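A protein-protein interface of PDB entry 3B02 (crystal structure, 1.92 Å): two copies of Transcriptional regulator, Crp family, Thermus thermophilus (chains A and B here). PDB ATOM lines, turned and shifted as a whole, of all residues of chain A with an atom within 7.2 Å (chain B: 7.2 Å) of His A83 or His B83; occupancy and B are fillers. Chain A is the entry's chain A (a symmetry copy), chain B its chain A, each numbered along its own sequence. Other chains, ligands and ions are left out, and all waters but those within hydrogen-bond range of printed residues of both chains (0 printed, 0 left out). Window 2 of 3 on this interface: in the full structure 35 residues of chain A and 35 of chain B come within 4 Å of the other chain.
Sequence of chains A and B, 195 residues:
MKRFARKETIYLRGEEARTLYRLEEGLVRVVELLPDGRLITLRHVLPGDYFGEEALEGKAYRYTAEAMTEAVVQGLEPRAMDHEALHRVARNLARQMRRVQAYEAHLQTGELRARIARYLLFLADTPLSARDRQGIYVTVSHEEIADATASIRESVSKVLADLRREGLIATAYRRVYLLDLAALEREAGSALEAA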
ATOM      1  N   ARG A  79     -10.637  19.523  21.626  1.00  0.00           N
ATOM      2  CA  ARG A  79      -9.681  19.327  22.704  1.00  0.00           C
ATOM      3  C   ARG A  79      -8.372  20.107  22.577  1.00  0.00           C
ATOM      4  O   ARG A  79      -7.592  20.159  23.523  1.00  0.00           O
ATOM      5  CB  ARG A  79      -9.387  17.830  22.835  1.00  0.00           C
ATOM      6  CG  ARG A  79     -10.648  16.974  22.727  1.00  0.00           C
ATOM      7  CD  ARG A  79     -10.371  15.488  22.892  1.00  0.00           C
ATOM      8  NE  ARG A  79     -11.432  14.665  22.308  1.00  0.00           N
ATOM      9  CZ  ARG A  79     -12.721  14.750  22.626  1.00  0.00           C
ATOM     10  NH1 ARG A  79     -13.135  15.627  23.533  1.00  0.00           N
ATOM     11  NH2 ARG A  79     -13.604  13.957  22.030  1.00  0.00           N
ATOM     12  N   ALA A  80      -8.139  20.723  21.423  1.00  0.00           N
ATOM     13  CA  ALA A  80      -6.898  21.466  21.210  1.00  0.00           C
ATOM     14  C   ALA A  80      -7.033  22.987  21.222  1.00  0.00           C
ATOM     15  O   ALA A  80      -6.132  23.692  20.766  1.00  0.00           O
ATOM     16  CB  ALA A  80      -6.254  21.019  19.904  1.00  0.00           C
ATOM     17  N   MET A  81      -8.144  23.496  21.745  1.00  0.00           N
ATOM     18  CA  MET A  81      -8.362  24.942  21.793  1.00  0.00           C
ATOM     19  C   MET A  81      -7.794  25.605  23.040  1.00  0.00           C
ATOM     20  O   MET A  81      -7.902  25.072  24.148  1.00  0.00           O
ATOM     21  CB  MET A  81      -9.855  25.260  21.703  1.00  0.00           C
ATOM     22  CG  MET A  81     -10.493  24.893  20.381  1.00  0.00           C
ATOM     23  SD  MET A  81     -12.227  25.371  20.339  1.00  0.00           S
ATOM     24  CE  MET A  81     -12.978  23.932  21.095  1.00  0.00           C
ATOM     25  N   ASP A  82      -7.195  26.778  22.855  1.00  0.00           N
ATOM     26  CA  ASP A  82      -6.626  27.517  23.972  1.00  0.00           C
ATOM     27  C   ASP A  82      -7.667  28.471  24.538  1.00  0.00           C
ATOM     28  O   ASP A  82      -8.789  28.552  24.033  1.00  0.00           O
ATOM     29  CB  ASP A  82      -5.384  28.307  23.534  1.00  0.00           C
ATOM     30  CG  ASP A  82      -5.725  29.533  22.705  1.00  0.00           C
ATOM     31  OD1 ASP A  82      -4.824  30.374  22.489  1.00  0.00           O
ATOM     32  OD2 ASP A  82      -6.884  29.661  22.264  1.00  0.00           O
ATOM     33  N   HIS A  83      -7.281  29.196  25.583  1.00  0.00           N
ATOM     34  CA  HIS A  83      -8.162  30.150  26.240  1.00  0.00           C
ATOM     35  C   HIS A  83      -8.822  31.094  25.235  1.00  0.00           C
ATOM     36  O   HIS A  83     -10.041  31.272  25.245  1.00  0.00           O
ATOM     37  CB  HIS A  83      -7.367  30.967  27.261  1.00  0.00           C
ATOM     38  CG  HIS A  83      -8.223  31.724  28.228  1.00  0.00           C
ATOM     39  ND1 HIS A  83      -8.906  31.109  29.255  1.00  0.00           N
ATOM     40  CD2 HIS A  83      -8.519  33.043  28.315  1.00  0.00           C
ATOM     41  CE1 HIS A  83      -9.587  32.014  29.934  1.00  0.00           C
ATOM     42  NE2 HIS A  83      -9.369  33.195  29.384  1.00  0.00           N
ATOM     43  N   GLU A  84      -8.008  31.694  24.374  1.00  0.00           N
ATOM     44  CA  GLU A  84      -8.498  32.632  23.370  1.00  0.00           C
ATOM     45  C   GLU A  84      -9.514  32.000  22.420  1.00  0.00           C
ATOM     46  O   GLU A  84     -10.508  32.630  22.057  1.00  0.00           O
ATOM     47  CB  GLU A  84      -7.324  33.191  22.568  1.00  0.00           C
ATOM     48  CG  GLU A  84      -7.714  34.222  21.527  1.00  0.00           C
ATOM     49  CD  GLU A  84      -6.519  34.742  20.753  1.00  0.00           C
ATOM     50  OE1 GLU A  84      -5.836  33.928  20.095  1.00  0.00           O
ATOM     51  OE2 GLU A  84      -6.263  35.963  20.806  1.00  0.00           O
ATOM     52  N   ALA A  85      -9.259  30.759  22.017  1.00  0.00           N
ATOM     53  CA  ALA A  85     -10.166  30.051  21.116  1.00  0.00           C
ATOM     54  C   ALA A  85     -11.495  29.766  21.815  1.00  0.00           C
ATOM     55  O   ALA A  85     -12.565  29.975  21.241  1.00  0.00           O
ATOM     56  CB  ALA A  85      -9.532  28.745  20.651  1.00  0.00           C
ATOM     57  N   LEU A  86     -11.422  29.291  23.056  1.00  0.00           N
ATOM     58  CA  LEU A  86     -12.627  28.983  23.815  1.00  0.00           C
ATOM     59  C   LEU A  86     -13.485  30.221  24.022  1.00  0.00           C
ATOM     60  O   LEU A  86     -14.713  30.144  24.015  1.00  0.00           O
ATOM     61  CB  LEU A  86     -12.263  28.373  25.171  1.00  0.00           C
ATOM     62  CG  LEU A  86     -11.808  26.912  25.149  1.00  0.00           C
ATOM     63  CD1 LEU A  86     -11.431  26.475  26.557  1.00  0.00           C
ATOM     64  CD2 LEU A  86     -12.922  26.034  24.598  1.00  0.00           C
ATOM     65  N   HIS A  87     -12.835  31.364  24.213  1.00  0.00           N
ATOM     66  CA  HIS A  87     -13.552  32.617  24.414  1.00  0.00           C
ATOM     67  C   HIS A  87     -14.338  32.932  23.141  1.00  0.00           C
ATOM     68  O   HIS A  87     -15.518  33.308  23.193  1.00  0.00           O
ATOM     69  CB  HIS A  87     -12.563  33.747  24.702  1.00  0.00           C
ATOM     70  CG  HIS A  87     -12.981  34.643  25.826  1.00  0.00           C
ATOM     71  ND1 HIS A  87     -13.104  34.196  27.124  1.00  0.00           N
ATOM     72  CD2 HIS A  87     -13.303  35.958  25.848  1.00  0.00           C
ATOM     73  CE1 HIS A  87     -13.487  35.195  27.897  1.00  0.00           C
ATOM     74  NE2 HIS A  87     -13.614  36.277  27.147  1.00  0.00           N
ATOM     75  N   ARG A  88     -13.681  32.773  21.995  1.00  0.00           N
ATOM     76  CA  ARG A  88     -14.337  33.037  20.722  1.00  0.00           C
ATOM     77  C   ARG A  88     -15.508  32.093  20.501  1.00  0.00           C
ATOM     78  O   ARG A  88     -16.559  32.514  20.015  1.00  0.00           O
ATOM     79  CB  ARG A  88     -13.358  32.904  19.552  1.00  0.00           C
ATOM     80  CG  ARG A  88     -12.471  34.111  19.343  1.00  0.00           C
ATOM     81  CD  ARG A  88     -11.970  34.166  17.907  1.00  0.00           C
ATOM     82  NE  ARG A  88     -11.277  32.943  17.511  1.00  0.00           N
ATOM     83  CZ  ARG A  88     -10.145  32.510  18.060  1.00  0.00           C
ATOM     84  NH1 ARG A  88      -9.568  33.201  19.034  1.00  0.00           N
ATOM     85  NH2 ARG A  88      -9.589  31.385  17.632  1.00  0.00           N
ATOM     86  N   VAL A  89     -15.327  30.822  20.849  1.00  0.00           N
ATOM     87  CA  VAL A  89     -16.389  29.834  20.676  1.00  0.00           C
ATOM     88  C   VAL A  89     -17.585  30.150  21.572  1.00  0.00           C
ATOM     89  O   VAL A  89     -18.735  30.122  21.125  1.00  0.00           O
ATOM     90  CB  VAL A  89     -15.889  28.404  20.978  1.00  0.00           C
ATOM     91  CG1 VAL A  89     -17.054  27.418  20.933  1.00  0.00           C
ATOM     92  CG2 VAL A  89     -14.823  28.005  19.960  1.00  0.00           C
ATOM     93  N   ARG B  79     -16.073  38.138  31.904  1.00  0.00           N
ATOM     94  CA  ARG B  79     -14.666  38.490  31.794  1.00  0.00           C
ATOM     95  C   ARG B  79     -13.745  37.855  32.836  1.00  0.00           C
ATOM     96  O   ARG B  79     -12.526  37.934  32.711  1.00  0.00           O
ATOM     97  CB  ARG B  79     -14.536  40.013  31.839  1.00  0.00           C
ATOM     98  CG  ARG B  79     -15.597  40.717  30.994  1.00  0.00           C
ATOM     99  CD  ARG B  79     -15.451  42.231  31.002  1.00  0.00           C
ATOM    100  NE  ARG B  79     -16.700  42.902  30.639  1.00  0.00           N
ATOM    101  CZ  ARG B  79     -17.379  42.688  29.513  1.00  0.00           C
ATOM    102  NH1 ARG B  79     -16.939  41.813  28.618  1.00  0.00           N
ATOM    103  NH2 ARG B  79     -18.507  43.349  29.285  1.00  0.00           N
ATOM    104  N   ALA B  80     -14.318  37.216  33.852  1.00  0.00           N
ATOM    105  CA  ALA B  80     -13.508  36.608  34.905  1.00  0.00           C
ATOM    106  C   ALA B  80     -13.425  35.084  34.872  1.00  0.00           C
ATOM    107  O   ALA B  80     -13.028  34.465  35.860  1.00  0.00           O
ATOM    108  CB  ALA B  80     -14.016  37.063  36.266  1.00  0.00           C
ATOM    109  N   MET B  81     -13.785  34.478  33.744  1.00  0.00           N
ATOM    110  CA  MET B  81     -13.744  33.022  33.625  1.00  0.00           C
ATOM    111  C   MET B  81     -12.396  32.484  33.164  1.00  0.00           C
ATOM    112  O   MET B  81     -11.758  33.051  32.273  1.00  0.00           O
ATOM    113  CB  MET B  81     -14.825  32.535  32.659  1.00  0.00           C
ATOM    114  CG  MET B  81     -16.242  32.766  33.140  1.00  0.00           C
ATOM    115  SD  MET B  81     -17.441  32.096  31.979  1.00  0.00           S
ATOM    116  CE  MET B  81     -17.603  33.475  30.848  1.00  0.00           C
ATOM    117  N   ASP B  82     -11.972  31.377  33.767  1.00  0.00           N
ATOM    118  CA  ASP B  82     -10.706  30.759  33.404  1.00  0.00           C
ATOM    119  C   ASP B  82     -10.939  29.721  32.316  1.00  0.00           C
ATOM    120  O   ASP B  82     -12.074  29.491  31.895  1.00  0.00           O
ATOM    121  CB  ASP B  82     -10.047  30.093  34.620  1.00  0.00           C
ATOM    122  CG  ASP B  82     -10.731  28.800  35.029  1.00  0.00           C
ATOM    123  OD1 ASP B  82     -10.152  28.057  35.852  1.00  0.00           O
ATOM    124  OD2 ASP B  82     -11.843  28.524  34.539  1.00  0.00           O
ATOM    125  N   HIS B  83      -9.853  29.094  31.874  1.00  0.00           N
ATOM    126  CA  HIS B  83      -9.908  28.079  30.832  1.00  0.00           C
ATOM    127  C   HIS B  83     -10.971  27.021  31.130  1.00  0.00           C
ATOM    128  O   HIS B  83     -11.806  26.708  30.280  1.00  0.00           O
ATOM    129  CB  HIS B  83      -8.542  27.402  30.698  1.00  0.00           C
ATOM    130  CG  HIS B  83      -8.386  26.600  29.444  1.00  0.00           C
ATOM    131  ND1 HIS B  83      -8.218  27.182  28.206  1.00  0.00           N
ATOM    132  CD2 HIS B  83      -8.386  25.262  29.235  1.00  0.00           C
ATOM    133  CE1 HIS B  83      -8.123  26.237  27.287  1.00  0.00           C
ATOM    134  NE2 HIS B  83      -8.222  25.064  27.886  1.00  0.00           N
ATOM    135  N   GLU B  84     -10.932  26.477  32.342  1.00  0.00           N
ATOM    136  CA  GLU B  84     -11.875  25.445  32.759  1.00  0.00           C
ATOM    137  C   GLU B  84     -13.328  25.915  32.696  1.00  0.00           C
ATOM    138  O   GLU B  84     -14.213  25.162  32.290  1.00  0.00           O
ATOM    139  CB  GLU B  84     -11.545  24.984  34.178  1.00  0.00           C
ATOM    140  CG  GLU B  84     -12.434  23.869  34.693  1.00  0.00           C
ATOM    141  CD  GLU B  84     -12.073  23.451  36.105  1.00  0.00           C
ATOM    142  OE1 GLU B  84     -12.142  24.306  37.015  1.00  0.00           O
ATOM    143  OE2 GLU B  84     -11.719  22.270  36.303  1.00  0.00           O
ATOM    144  N   ALA B  85     -13.569  27.156  33.105  1.00  0.00           N
ATOM    145  CA  ALA B  85     -14.919  27.717  33.081  1.00  0.00           C
ATOM    146  C   ALA B  85     -15.400  27.883  31.640  1.00  0.00           C
ATOM    147  O   ALA B  85     -16.533  27.529  31.310  1.00  0.00           O
ATOM    148  CB  ALA B  85     -14.942  29.062  33.796  1.00  0.00           C
ATOM    149  N   LEU B  86     -14.534  28.420  30.783  1.00  0.00           N
ATOM    150  CA  LEU B  86     -14.887  28.625  29.385  1.00  0.00           C
ATOM    151  C   LEU B  86     -15.209  27.309  28.694  1.00  0.00           C
ATOM    152  O   LEU B  86     -16.090  27.249  27.837  1.00  0.00           O
ATOM    153  CB  LEU B  86     -13.751  29.334  28.645  1.00  0.00           C
ATOM    154  CG  LEU B  86     -13.608  30.834  28.912  1.00  0.00           C
ATOM    155  CD1 LEU B  86     -12.407  31.374  28.151  1.00  0.00           C
ATOM    156  CD2 LEU B  86     -14.877  31.555  28.485  1.00  0.00           C
ATOM    157  N   HIS B  87     -14.490  26.256  29.065  1.00  0.00           N
ATOM    158  CA  HIS B  87     -14.715  24.942  28.478  1.00  0.00           C
ATOM    159  C   HIS B  87     -16.125  24.482  28.851  1.00  0.00           C
ATOM    160  O   HIS B  87     -16.879  23.980  28.006  1.00  0.00           O
ATOM    161  CB  HIS B  87     -13.689  23.943  29.017  1.00  0.00           C
ATOM    162  CG  HIS B  87     -13.097  23.059  27.964  1.00  0.00           C
ATOM    163  ND1 HIS B  87     -12.327  23.549  26.931  1.00  0.00           N
ATOM    164  CD2 HIS B  87     -13.162  21.720  27.784  1.00  0.00           C
ATOM    165  CE1 HIS B  87     -11.943  22.549  26.158  1.00  0.00           C
ATOM    166  NE2 HIS B  87     -12.436  21.427  26.654  1.00  0.00           N
ATOM    167  N   ARG B  88     -16.481  24.661  30.120  1.00  0.00           N
ATOM    168  CA  ARG B  88     -17.804  24.267  30.581  1.00  0.00           C
ATOM    169  C   ARG B  88     -18.891  25.063  29.877  1.00  0.00           C
ATOM    170  O   ARG B  88     -19.924  24.505  29.508  1.00  0.00           O
ATOM    171  CB  ARG B  88     -17.946  24.455  32.093  1.00  0.00           C
ATOM    172  CG  ARG B  88     -17.330  23.346  32.920  1.00  0.00           C
ATOM    173  CD  ARG B  88     -17.976  23.281  34.297  1.00  0.00           C
ATOM    174  NE  ARG B  88     -17.901  24.555  35.007  1.00  0.00           N
ATOM    175  CZ  ARG B  88     -16.767  25.137  35.388  1.00  0.00           C
ATOM    176  NH1 ARG B  88     -15.600  24.560  35.129  1.00  0.00           N
ATOM    177  NH2 ARG B  88     -16.800  26.297  36.031  1.00  0.00           N
ATOM    178  N   VAL B  89     -18.662  26.362  29.696  1.00  0.00           N
ATOM    179  CA  VAL B  89     -19.644  27.215  29.032  1.00  0.00           C
ATOM    180  C   VAL B  89     -19.824  26.808  27.570  1.00  0.00           C
ATOM    181  O   VAL B  89     -20.953  26.686  27.083  1.00  0.00           O
ATOM    182  CB  VAL B  89     -19.239  28.705  29.100  1.00  0.00           C
ATOM    183  CG1 VAL B  89     -20.203  29.551  28.273  1.00  0.00           C
ATOM    184  CG2 VAL B  89     -19.244  29.173  30.553  1.00  0.00           C
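A ring nitrogen (ND1) of His B83 lies within hydrogen-bond range of the backbone NH of His A83.
The side-chain carboxylate (OD2) of Asp A82 is in hydrogen-bond range of the backbone NH (N) of Glu A84.
The backbone NH (N) of Ala A85 sits at hydrogen-bond distance from the side-chain carboxylate (OD2) of Asp A82, 2.6 Å away.
The backbone NH of Glu B84 lies within hydrogen-bond range of the side-chain carboxylate of Asp B82 (3.1 Å).
OD2 of Asp B82 sits at hydrogen-bond distance from N of Ala B85 (2.6 Å).
Met A81 touches His B83 (O to CE1, 3.4 Å).
Asp A82 touches His B83.
CE1 of His A83 touches O of Met B81 (3.4 Å).
Asp B82 touches His A83.
His A83 touches Leu B86.
Leu A86 touches His B83.
Leu B86 touches Leu A86.
Leu A86 touches His B87.
His A87 touches Leu B86 (ND1 to CD1, 3.1 Å).
Of chain B, only Met B81, Asp B82, His B83 and Leu B86 come within 4 Å of His A83.
Val A89 touches none of the printed residues of chain B.
Of the printed residues of chain A, Met B81 touches His A83.
His B83 touches just these residues of chain A: Met A81, Asp A82, His A83 and Leu A86.
Ala B85 touches none of the printed residues of chain A.
Of the printed residues of chain A, Leu B86 touches His A83 (3.4 Å), Leu A86 (3.9 Å) and His A87 (3.1 Å).
Of the printed residues of chain A, His B87 touches Leu A86 (3.1 Å).
The nearest residue of chain B that does not touch His A83 is Glu B84 (5.9 Å).
The nearest residue of chain A that does not touch His B83 is Glu A84 (5.9 Å).
Hydrophobic or aromatic side chains of chain B that line the printed part of chain A: His B83, Leu B86 and His B87.
Printed residues of chain A that touch a printed residue of chain B: Met A81, Asp A82, His A83, Leu A86 and His A87.
Hydrophobic or aromatic side chains of chain A that line the printed part of chain B: His A83, Leu A86 and His A87.
Asp A82 touches His B83, and with the chains exchanged His A83 touches Asp B82.
His A83 touches its own counterpart, His B83.
Leu A86 touches its own counterpart, Leu B86.
Leu A86 touches His B87, and with the chains exchanged His A87 touches Leu B86.
Of the 10 pairs that touch across the chains among the printed residues, 10 have their exchanged pair printed and touching as well.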
